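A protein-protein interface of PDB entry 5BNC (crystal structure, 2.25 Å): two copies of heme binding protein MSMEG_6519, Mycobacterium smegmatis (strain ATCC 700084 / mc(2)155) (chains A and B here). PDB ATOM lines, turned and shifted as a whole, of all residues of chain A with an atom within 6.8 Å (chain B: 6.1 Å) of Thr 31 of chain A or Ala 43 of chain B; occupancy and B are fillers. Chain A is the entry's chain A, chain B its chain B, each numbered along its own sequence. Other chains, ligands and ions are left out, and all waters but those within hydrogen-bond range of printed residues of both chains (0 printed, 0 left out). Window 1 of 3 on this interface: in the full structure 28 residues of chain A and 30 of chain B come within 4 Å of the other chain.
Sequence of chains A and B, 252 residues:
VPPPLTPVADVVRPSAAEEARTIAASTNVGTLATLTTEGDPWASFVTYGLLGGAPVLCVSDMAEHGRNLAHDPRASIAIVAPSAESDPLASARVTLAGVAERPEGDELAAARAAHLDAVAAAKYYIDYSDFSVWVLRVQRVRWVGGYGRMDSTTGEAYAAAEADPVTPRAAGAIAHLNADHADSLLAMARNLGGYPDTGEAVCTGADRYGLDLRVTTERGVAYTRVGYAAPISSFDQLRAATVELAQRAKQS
The side-chain hydroxyl (OG1) of Thr 95 of chain A is in hydrogen-bond range of the backbone carbonyl oxygen (O) of Ala 43 of chain B. The side-chain hydroxyl of Ser 76 of chain A sits at hydrogen-bond distance from the backbone NH of Ala 43 of chain B (2.8 Å). OG of Ser 76 of chain A is in hydrogen-bond range of O of Pro 41 of chain B (2.7 Å). The side-chain hydroxyl (OG1) of Thr 31 of chain B sits at hydrogen-bond distance from the side-chain hydroxyl (OG1) of Thr 31 of chain A (3.5 Å).
O of Thr 31 of chain A lies within hydrogen-bond range of N of Ala 78 of chain A, at 3.0 Å. NE1 of Trp 42 of chain A lies close to OG of Ser 44 of chain A (3.2 Å). N of Ala 33 of chain A is in hydrogen-bond range of O of Ser 76 of chain A. O of Thr 31 of chain B lies within hydrogen-bond range of N of Ala 78 of chain B (3.0 Å). The indole nitrogen of Trp 42 of chain B lies close to the side-chain hydroxyl of Ser 44 of chain B. O of Thr 34 of chain B lies within hydrogen-bond range of N of Trp 42 of chain B, 2.8 Å away.
Among the printed residues, pairs that only touch across the chains: Thr 31 of chain A with Ala 43 of chain B (3.8 Å), Thr 31 of chain A with Ala 78 of chain B (3.7 Å), Ala 33 of chain A with Ala 33 of chain B (3.98 Å), Ala 33 of chain A with Pro 41 of chain B (3.5 Å), Ala 33 of chain A with Trp 42 of chain B (3.8 Å), Ala 33 of chain A with Ala 43 of chain B (3.6 Å), Trp 42 of chain A with Ala 33 of chain B (3.9 Å), Ala 43 of chain A with Thr 31 of chain B (3.8 Å), Ala 43 of chain A with Ala 33 of chain B (3.7 Å), Ala 43 of chain A with Ala 78 of chain B (3.6 Å), Phe 45 of chain A with Val 80 of chain B (3.7 Å), Ala 75 of chain A with Pro 41 of chain B (3.8 Å), Ser 76 of chain A with Trp 42 of chain B (3.4 Å), Ala 78 of chain A with Thr 31 of chain B (3.6 Å), Ala 78 of chain A with Ala 43 of chain B (3.7 Å) and Thr 95 of chain A with Trp 42 of chain B (3.8 Å).
Of chain B, only Thr 31 (3.5 Å), Ala 43 (3.8 Å) and Ala 78 (3.7 Å) come within 4 Å of Thr 31 of chain A. Of the printed residues of chain A, Ala 43 of chain B touches Thr 31 (3.8 Å), Ala 33 (3.6 Å), Ser 76 (2.8 Å), Ala 78 (3.7 Å) and Thr 95 (2.6 Å). Of the printed residues of chain B, Ala 33 of chain A touches Ala 33 (3.98 Å), Pro 41 (3.5 Å), Trp 42 (3.8 Å) and Ala 43 (3.6 Å). Of the printed residues of chain A, Pro 41 of chain B touches Ala 33, Ala 75 and Ser 76. Of the printed residues of chain B, Ala 78 of chain A touches Thr 31 (3.6 Å) and Ala 43 (3.7 Å). Of the printed residues of chain B, Phe 45 of chain A touches Val 80. Of the printed residues of chain B, Ala 75 of chain A touches Pro 41 (3.8 Å). Leu 96 of chain A touches none of the printed residues of chain B. The nearest residue of chain A that does not touch Ala 43 of chain B is Ile 77 of chain A (4.1 Å).
Of the 19 printed residues of chain A, 9 touch a printed residue of chain B. Among the printed residues, no Asp or Glu carboxylate lies within 4 Å of a Lys or Arg side-chain nitrogen of the other chain.
Thr 31 of chain A touches its own counterpart, Thr 31 of chain B. Thr 31 of chain A touches Ala 78 of chain B, and with the chains exchanged Ala 78 of chain A touches Thr 31 of chain B. Ala 33 of chain A touches Trp 42 of chain B, and with the chains exchanged Trp 42 of chain A touches Ala 33 of chain B. Ala 43 of chain A touches Ala 78 of chain B, and with the chains exchanged Ala 78 of chain A touches Ala 43 of chain B. Of the 20 pairs that touch across the chains among the printed residues, 12 have their exchanged pair printed and touching as well.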
ATOM      1  N   VAL A  29     -32.629  15.524   7.857  1.00  0.00           N
ATOM      2  CA  VAL A  29     -32.037  16.137   6.676  1.00  0.00           C
ATOM      3  C   VAL A  29     -30.838  16.951   7.052  1.00  0.00           C
ATOM      4  O   VAL A  29     -30.787  17.571   8.127  1.00  0.00           O
ATOM      5  CB  VAL A  29     -33.017  17.014   5.890  1.00  0.00           C
ATOM      6  CG1 VAL A  29     -34.123  16.159   5.289  1.00  0.00           C
ATOM      7  CG2 VAL A  29     -33.621  18.090   6.782  1.00  0.00           C
ATOM      8  N   GLY A  30     -29.825  16.885   6.201  1.00  0.00           N
ATOM      9  CA  GLY A  30     -28.727  17.812   6.293  1.00  0.00           C
ATOM     10  C   GLY A  30     -28.034  17.897   4.983  1.00  0.00           C
ATOM     11  O   GLY A  30     -28.582  17.474   3.973  1.00  0.00           O
ATOM     12  N   THR A  31     -26.836  18.456   5.003  1.00  0.00           N
ATOM     13  CA  THR A  31     -26.049  18.592   3.808  1.00  0.00           C
ATOM     14  C   THR A  31     -24.664  17.990   4.010  1.00  0.00           C
ATOM     15  O   THR A  31     -23.914  18.378   4.922  1.00  0.00           O
ATOM     16  CB  THR A  31     -25.928  20.067   3.389  1.00  0.00           C
ATOM     17  OG1 THR A  31     -27.237  20.540   3.074  1.00  0.00           O
ATOM     18  CG2 THR A  31     -25.066  20.239   2.131  1.00  0.00           C
ATOM     19  N   LEU A  32     -24.317  17.052   3.142  1.00  0.00           N
ATOM     20  CA  LEU A  32     -23.009  16.384   3.223  1.00  0.00           C
ATOM     21  C   LEU A  32     -21.985  17.182   2.446  1.00  0.00           C
ATOM     22  O   LEU A  32     -22.300  17.788   1.433  1.00  0.00           O
ATOM     23  CB  LEU A  32     -23.105  15.007   2.613  1.00  0.00           C
ATOM     24  CG  LEU A  32     -22.051  13.962   2.913  1.00  0.00           C
ATOM     25  CD1 LEU A  32     -22.054  13.542   4.376  1.00  0.00           C
ATOM     26  CD2 LEU A  32     -22.339  12.777   1.992  1.00  0.00           C
ATOM     27  N   ALA A  33     -20.761  17.201   2.952  1.00  0.00           N
ATOM     28  CA  ALA A  33     -19.639  17.749   2.192  1.00  0.00           C
ATOM     29  C   ALA A  33     -18.727  16.592   1.900  1.00  0.00           C
ATOM     30  O   ALA A  33     -18.319  15.852   2.818  1.00  0.00           O
ATOM     31  CB  ALA A  33     -18.903  18.862   2.962  1.00  0.00           C
ATOM     32  N   TRP A  42     -17.682  19.341  -2.480  1.00  0.00           N
ATOM     33  CA  TRP A  42     -19.028  19.092  -3.054  1.00  0.00           C
ATOM     34  C   TRP A  42     -20.113  19.022  -1.970  1.00  0.00           C
ATOM     35  O   TRP A  42     -20.054  18.153  -1.134  1.00  0.00           O
ATOM     36  CB  TRP A  42     -19.054  17.723  -3.778  1.00  0.00           C
ATOM     37  CG  TRP A  42     -20.294  17.510  -4.564  1.00  0.00           C
ATOM     38  CD1 TRP A  42     -21.308  16.641  -4.302  1.00  0.00           C
ATOM     39  CD2 TRP A  42     -20.692  18.259  -5.697  1.00  0.00           C
ATOM     40  NE1 TRP A  42     -22.314  16.786  -5.251  1.00  0.00           N
ATOM     41  CE2 TRP A  42     -21.949  17.778  -6.106  1.00  0.00           C
ATOM     42  CE3 TRP A  42     -20.094  19.280  -6.431  1.00  0.00           C
ATOM     43  CZ2 TRP A  42     -22.600  18.280  -7.201  1.00  0.00           C
ATOM     44  CZ3 TRP A  42     -20.738  19.760  -7.518  1.00  0.00           C
ATOM     45  CH2 TRP A  42     -21.980  19.272  -7.888  1.00  0.00           C
ATOM     46  N   ALA A  43     -21.064  19.943  -1.993  1.00  0.00           N
ATOM     47  CA  ALA A  43     -22.184  19.985  -1.020  1.00  0.00           C
ATOM     48  C   ALA A  43     -23.369  19.227  -1.592  1.00  0.00           C
ATOM     49  O   ALA A  43     -23.849  19.570  -2.684  1.00  0.00           O
ATOM     50  CB  ALA A  43     -22.586  21.424  -0.746  1.00  0.00           C
ATOM     51  N   SER A  44     -23.888  18.261  -0.835  1.00  0.00           N
ATOM     52  CA  SER A  44     -25.100  17.497  -1.231  1.00  0.00           C
ATOM     53  C   SER A  44     -26.170  17.449  -0.138  1.00  0.00           C
ATOM     54  O   SER A  44     -25.888  17.116   1.010  1.00  0.00           O
ATOM     55  CB  SER A  44     -24.729  16.035  -1.542  1.00  0.00           C
ATOM     56  OG  SER A  44     -23.590  15.928  -2.389  1.00  0.00           O
ATOM     57  N   PHE A  45     -27.410  17.710  -0.499  1.00  0.00           N
ATOM     58  CA  PHE A  45     -28.531  17.432   0.356  1.00  0.00           C
ATOM     59  C   PHE A  45     -28.572  15.916   0.624  1.00  0.00           C
ATOM     60  O   PHE A  45     -28.454  15.112  -0.312  1.00  0.00           O
ATOM     61  CB  PHE A  45     -29.812  17.878  -0.338  1.00  0.00           C
ATOM     62  CG  PHE A  45     -31.085  17.435   0.348  1.00  0.00           C
ATOM     63  CD1 PHE A  45     -31.478  17.994   1.546  1.00  0.00           C
ATOM     64  CD2 PHE A  45     -31.909  16.493  -0.238  1.00  0.00           C
ATOM     65  CE1 PHE A  45     -32.672  17.605   2.153  1.00  0.00           C
ATOM     66  CE2 PHE A  45     -33.105  16.117   0.364  1.00  0.00           C
ATOM     67  CZ  PHE A  45     -33.484  16.663   1.561  1.00  0.00           C
ATOM     68  N   VAL A  46     -28.753  15.521   1.876  1.00  0.00           N
ATOM     69  CA  VAL A  46     -28.929  14.118   2.240  1.00  0.00           C
ATOM     70  C   VAL A  46     -29.943  13.926   3.351  1.00  0.00           C
ATOM     71  O   VAL A  46     -30.150  14.818   4.185  1.00  0.00           O
ATOM     72  CB  VAL A  46     -27.619  13.472   2.705  1.00  0.00           C
ATOM     73  CG1 VAL A  46     -26.594  13.495   1.596  1.00  0.00           C
ATOM     74  CG2 VAL A  46     -27.041  14.188   3.929  1.00  0.00           C
ATOM     75  N   TYR A  48     -30.895  11.147   6.643  1.00  0.00           N
ATOM     76  CA  TYR A  48     -30.114  10.262   7.539  1.00  0.00           C
ATOM     77  C   TYR A  48     -30.893   9.819   8.731  1.00  0.00           C
ATOM     78  O   TYR A  48     -31.843  10.501   9.156  1.00  0.00           O
ATOM     79  CB  TYR A  48     -28.807  10.936   8.040  1.00  0.00           C
ATOM     80  CG  TYR A  48     -29.057  12.089   8.993  1.00  0.00           C
ATOM     81  CD1 TYR A  48     -29.166  11.878  10.353  1.00  0.00           C
ATOM     82  CD2 TYR A  48     -29.250  13.370   8.527  1.00  0.00           C
ATOM     83  CE1 TYR A  48     -29.455  12.909  11.205  1.00  0.00           C
ATOM     84  CE2 TYR A  48     -29.512  14.412   9.387  1.00  0.00           C
ATOM     85  CZ  TYR A  48     -29.627  14.158  10.726  1.00  0.00           C
ATOM     86  OH  TYR A  48     -29.908  15.169  11.578  1.00  0.00           O
ATOM     87  N   ALA A  75     -15.773  12.865   4.940  1.00  0.00           N
ATOM     88  CA  ALA A  75     -17.028  13.556   4.794  1.00  0.00           C
ATOM     89  C   ALA A  75     -17.333  14.371   6.053  1.00  0.00           C
ATOM     90  O   ALA A  75     -16.831  14.062   7.140  1.00  0.00           O
ATOM     91  CB  ALA A  75     -18.121  12.555   4.562  1.00  0.00           C
ATOM     92  N   SER A  76     -18.107  15.440   5.897  1.00  0.00           N
ATOM     93  CA  SER A  76     -18.734  16.085   7.042  1.00  0.00           C
ATOM     94  C   SER A  76     -20.195  16.388   6.702  1.00  0.00           C
ATOM     95  O   SER A  76     -20.574  16.404   5.537  1.00  0.00           O
ATOM     96  CB  SER A  76     -17.947  17.324   7.466  1.00  0.00           C
ATOM     97  OG  SER A  76     -17.938  18.305   6.445  1.00  0.00           O
ATOM     98  N   ILE A  77     -21.023  16.602   7.709  1.00  0.00           N
ATOM     99  CA  ILE A  77     -22.423  16.927   7.485  1.00  0.00           C
ATOM    100  C   ILE A  77     -22.809  18.116   8.395  1.00  0.00           C
ATOM    101  O   ILE A  77     -22.410  18.168   9.577  1.00  0.00           O
ATOM    102  CB  ILE A  77     -23.289  15.714   7.722  1.00  0.00           C
ATOM    103  CG1 ILE A  77     -24.733  15.977   7.337  1.00  0.00           C
ATOM    104  CG2 ILE A  77     -23.258  15.285   9.176  1.00  0.00           C
ATOM    105  CD1 ILE A  77     -25.645  14.795   7.511  1.00  0.00           C
ATOM    106  N   ALA A  78     -23.509  19.098   7.826  1.00  0.00           N
ATOM    107  CA  ALA A  78     -24.035  20.192   8.610  1.00  0.00           C
ATOM    108  C   ALA A  78     -25.515  19.919   8.819  1.00  0.00           C
ATOM    109  O   ALA A  78     -26.204  19.546   7.892  1.00  0.00           O
ATOM    110  CB  ALA A  78     -23.860  21.537   7.909  1.00  0.00           C
ATOM    111  N   ILE A  79     -25.960  20.135  10.041  1.00  0.00           N
ATOM    112  CA  ILE A  79     -27.317  19.822  10.466  1.00  0.00           C
ATOM    113  C   ILE A  79     -27.833  21.044  11.215  1.00  0.00           C
ATOM    114  O   ILE A  79     -27.146  21.589  12.048  1.00  0.00           O
ATOM    115  CB  ILE A  79     -27.355  18.580  11.393  1.00  0.00           C
ATOM    116  CG1 ILE A  79     -26.803  17.323  10.695  1.00  0.00           C
ATOM    117  CG2 ILE A  79     -28.787  18.294  11.822  1.00  0.00           C
ATOM    118  CD1 ILE A  79     -26.550  16.142  11.611  1.00  0.00           C
ATOM    119  N   VAL A  94     -24.778  22.334  13.622  1.00  0.00           N
ATOM    120  CA  VAL A  94     -23.623  21.570  13.911  1.00  0.00           C
ATOM    121  C   VAL A  94     -22.987  21.005  12.644  1.00  0.00           C
ATOM    122  O   VAL A  94     -23.671  20.692  11.687  1.00  0.00           O
ATOM    123  CB  VAL A  94     -24.004  20.472  14.906  1.00  0.00           C
ATOM    124  CG1 VAL A  94     -24.820  19.371  14.237  1.00  0.00           C
ATOM    125  CG2 VAL A  94     -22.785  19.900  15.568  1.00  0.00           C
ATOM    126  N   THR A  95     -21.651  20.955  12.621  1.00  0.00           N
ATOM    127  CA  THR A  95     -20.908  20.134  11.648  1.00  0.00           C
ATOM    128  C   THR A  95     -20.324  18.902  12.372  1.00  0.00           C
ATOM    129  O   THR A  95     -19.635  19.035  13.368  1.00  0.00           O
ATOM    130  CB  THR A  95     -19.768  20.940  11.001  1.00  0.00           C
ATOM    131  OG1 THR A  95     -20.319  22.129  10.400  1.00  0.00           O
ATOM    132  CG2 THR A  95     -19.055  20.136   9.903  1.00  0.00           C
ATOM    133  N   LEU A  96     -20.661  17.734  11.872  1.00  0.00           N
ATOM    134  CA  LEU A  96     -20.078  16.510  12.293  1.00  0.00           C
ATOM    135  C   LEU A  96     -19.132  16.083  11.187  1.00  0.00           C
ATOM    136  O   LEU A  96     -19.536  15.943  10.052  1.00  0.00           O
ATOM    137  CB  LEU A  96     -21.161  15.452  12.481  1.00  0.00           C
ATOM    138  CG  LEU A  96     -22.307  15.763  13.444  1.00  0.00           C
ATOM    139  CD1 LEU A  96     -23.302  14.635  13.604  1.00  0.00           C
ATOM    140  CD2 LEU A  96     -21.831  16.186  14.815  1.00  0.00           C
ATOM    141  N   GLY B  30     -28.340  28.106   3.172  1.00  0.00           N
ATOM    142  CA  GLY B  30     -27.901  26.837   2.633  1.00  0.00           C
ATOM    143  C   GLY B  30     -26.678  26.352   3.394  1.00  0.00           C
ATOM    144  O   GLY B  30     -26.397  26.816   4.487  1.00  0.00           O
ATOM    145  N   THR B  31     -25.963  25.420   2.802  1.00  0.00           N
ATOM    146  CA  THR B  31     -24.784  24.845   3.419  1.00  0.00           C
ATOM    147  C   THR B  31     -23.588  24.928   2.444  1.00  0.00           C
ATOM    148  O   THR B  31     -23.642  24.444   1.324  1.00  0.00           O
ATOM    149  CB  THR B  31     -25.034  23.416   3.838  1.00  0.00           C
ATOM    150  OG1 THR B  31     -26.129  23.401   4.719  1.00  0.00           O
ATOM    151  CG2 THR B  31     -23.801  22.817   4.536  1.00  0.00           C
ATOM    152  N   LEU B  32     -22.540  25.586   2.893  1.00  0.00           N
ATOM    153  CA  LEU B  32     -21.315  25.746   2.088  1.00  0.00           C
ATOM    154  C   LEU B  32     -20.437  24.532   2.277  1.00  0.00           C
ATOM    155  O   LEU B  32     -20.365  23.973   3.374  1.00  0.00           O
ATOM    156  CB  LEU B  32     -20.588  26.981   2.544  1.00  0.00           C
ATOM    157  CG  LEU B  32     -19.537  27.556   1.616  1.00  0.00           C
ATOM    158  CD1 LEU B  32     -20.145  28.142   0.337  1.00  0.00           C
ATOM    159  CD2 LEU B  32     -18.831  28.628   2.432  1.00  0.00           C
ATOM    160  N   ALA B  33     -19.813  24.080   1.200  1.00  0.00           N
ATOM    161  CA  ALA B  33     -18.762  23.060   1.303  1.00  0.00           C
ATOM    162  C   ALA B  33     -17.458  23.771   0.936  1.00  0.00           C
ATOM    163  O   ALA B  33     -17.355  24.435  -0.111  1.00  0.00           O
ATOM    164  CB  ALA B  33     -19.004  21.885   0.380  1.00  0.00           C
ATOM    165  N   THR B  34     -16.490  23.643   1.830  1.00  0.00           N
ATOM    166  CA  THR B  34     -15.162  24.177   1.628  1.00  0.00           C
ATOM    167  C   THR B  34     -14.131  23.117   2.035  1.00  0.00           C
ATOM    168  O   THR B  34     -14.480  22.034   2.483  1.00  0.00           O
ATOM    169  CB  THR B  34     -14.925  25.473   2.437  1.00  0.00           C
ATOM    170  OG1 THR B  34     -15.060  25.199   3.835  1.00  0.00           O
ATOM    171  CG2 THR B  34     -15.904  26.539   2.041  1.00  0.00           C
ATOM    172  N   PRO B  41     -13.217  17.709   3.522  1.00  0.00           N
ATOM    173  CA  PRO B  41     -14.429  18.442   3.138  1.00  0.00           C
ATOM    174  C   PRO B  41     -15.172  18.959   4.383  1.00  0.00           C
ATOM    175  O   PRO B  41     -15.468  18.175   5.281  1.00  0.00           O
ATOM    176  CB  PRO B  41     -15.220  17.387   2.337  1.00  0.00           C
ATOM    177  CG  PRO B  41     -14.850  16.090   2.961  1.00  0.00           C
ATOM    178  CD  PRO B  41     -13.401  16.247   3.395  1.00  0.00           C
ATOM    179  N   TRP B  42     -15.401  20.272   4.429  1.00  0.00           N
ATOM    180  CA  TRP B  42     -16.023  20.945   5.560  1.00  0.00           C
ATOM    181  C   TRP B  42     -17.387  21.510   5.167  1.00  0.00           C
ATOM    182  O   TRP B  42     -17.452  22.427   4.333  1.00  0.00           O
ATOM    183  CB  TRP B  42     -15.155  22.124   6.027  1.00  0.00           C
ATOM    184  CG  TRP B  42     -15.624  22.707   7.343  1.00  0.00           C
ATOM    185  CD1 TRP B  42     -16.164  23.948   7.572  1.00  0.00           C
ATOM    186  CD2 TRP B  42     -15.594  22.048   8.604  1.00  0.00           C
ATOM    187  NE1 TRP B  42     -16.471  24.100   8.934  1.00  0.00           N
ATOM    188  CE2 TRP B  42     -16.121  22.945   9.576  1.00  0.00           C
ATOM    189  CE3 TRP B  42     -15.131  20.788   9.020  1.00  0.00           C
ATOM    190  CZ2 TRP B  42     -16.220  22.604  10.918  1.00  0.00           C
ATOM    191  CZ3 TRP B  42     -15.239  20.443  10.346  1.00  0.00           C
ATOM    192  CH2 TRP B  42     -15.774  21.350  11.288  1.00  0.00           C
ATOM    193  N   ALA B  43     -18.459  21.013   5.790  1.00  0.00           N
ATOM    194  CA  ALA B  43     -19.837  21.555   5.588  1.00  0.00           C
ATOM    195  C   ALA B  43     -20.160  22.618   6.615  1.00  0.00           C
ATOM    196  O   ALA B  43     -20.026  22.357   7.790  1.00  0.00           O
ATOM    197  CB  ALA B  43     -20.857  20.430   5.699  1.00  0.00           C
ATOM    198  N   SER B  44     -20.634  23.787   6.177  1.00  0.00           N
ATOM    199  CA  SER B  44     -21.028  24.904   7.057  1.00  0.00           C
ATOM    200  C   SER B  44     -22.381  25.544   6.713  1.00  0.00           C
ATOM    201  O   SER B  44     -22.631  25.894   5.569  1.00  0.00           O
ATOM    202  CB  SER B  44     -20.019  26.099   6.942  1.00  0.00           C
ATOM    203  OG  SER B  44     -18.703  25.708   7.097  1.00  0.00           O
ATOM    204  N   PHE B  45     -23.200  25.781   7.727  1.00  0.00           N
ATOM    205  CA  PHE B  45     -24.438  26.520   7.582  1.00  0.00           C
ATOM    206  C   PHE B  45     -24.085  27.934   7.218  1.00  0.00           C
ATOM    207  O   PHE B  45     -23.172  28.516   7.838  1.00  0.00           O
ATOM    208  CB  PHE B  45     -25.213  26.493   8.920  1.00  0.00           C
ATOM    209  CG  PHE B  45     -26.382  27.443   8.974  1.00  0.00           C
ATOM    210  CD1 PHE B  45     -27.510  27.224   8.209  1.00  0.00           C
ATOM    211  CD2 PHE B  45     -26.357  28.570   9.793  1.00  0.00           C
ATOM    212  CE1 PHE B  45     -28.609  28.094   8.272  1.00  0.00           C
ATOM    213  CE2 PHE B  45     -27.428  29.476   9.800  1.00  0.00           C
ATOM    214  CZ  PHE B  45     -28.545  29.232   9.040  1.00  0.00           C
ATOM    215  N   ALA B  78     -25.090  23.941  -1.300  1.00  0.00           N
ATOM    216  CA  ALA B  78     -26.338  23.230  -1.570  1.00  0.00           C
ATOM    217  C   ALA B  78     -27.471  24.022  -1.001  1.00  0.00           C
ATOM    218  O   ALA B  78     -27.386  24.497   0.142  1.00  0.00           O
ATOM    219  CB  ALA B  78     -26.330  21.842  -0.942  1.00  0.00           C
ATOM    220  N   VAL B  80     -31.840  24.217  -0.670  1.00  0.00           N
ATOM    221  CA  VAL B  80     -33.038  23.430  -0.638  1.00  0.00           C
ATOM    222  C   VAL B  80     -34.249  24.398  -0.563  1.00  0.00           C
ATOM    223  O   VAL B  80     -34.306  25.220   0.320  1.00  0.00           O
ATOM    224  CB  VAL B  80     -33.017  22.407   0.550  1.00  0.00           C
ATOM    225  CG1 VAL B  80     -34.282  21.536   0.539  1.00  0.00           C
ATOM    226  CG2 VAL B  80     -31.782  21.517   0.464  1.00  0.00           C
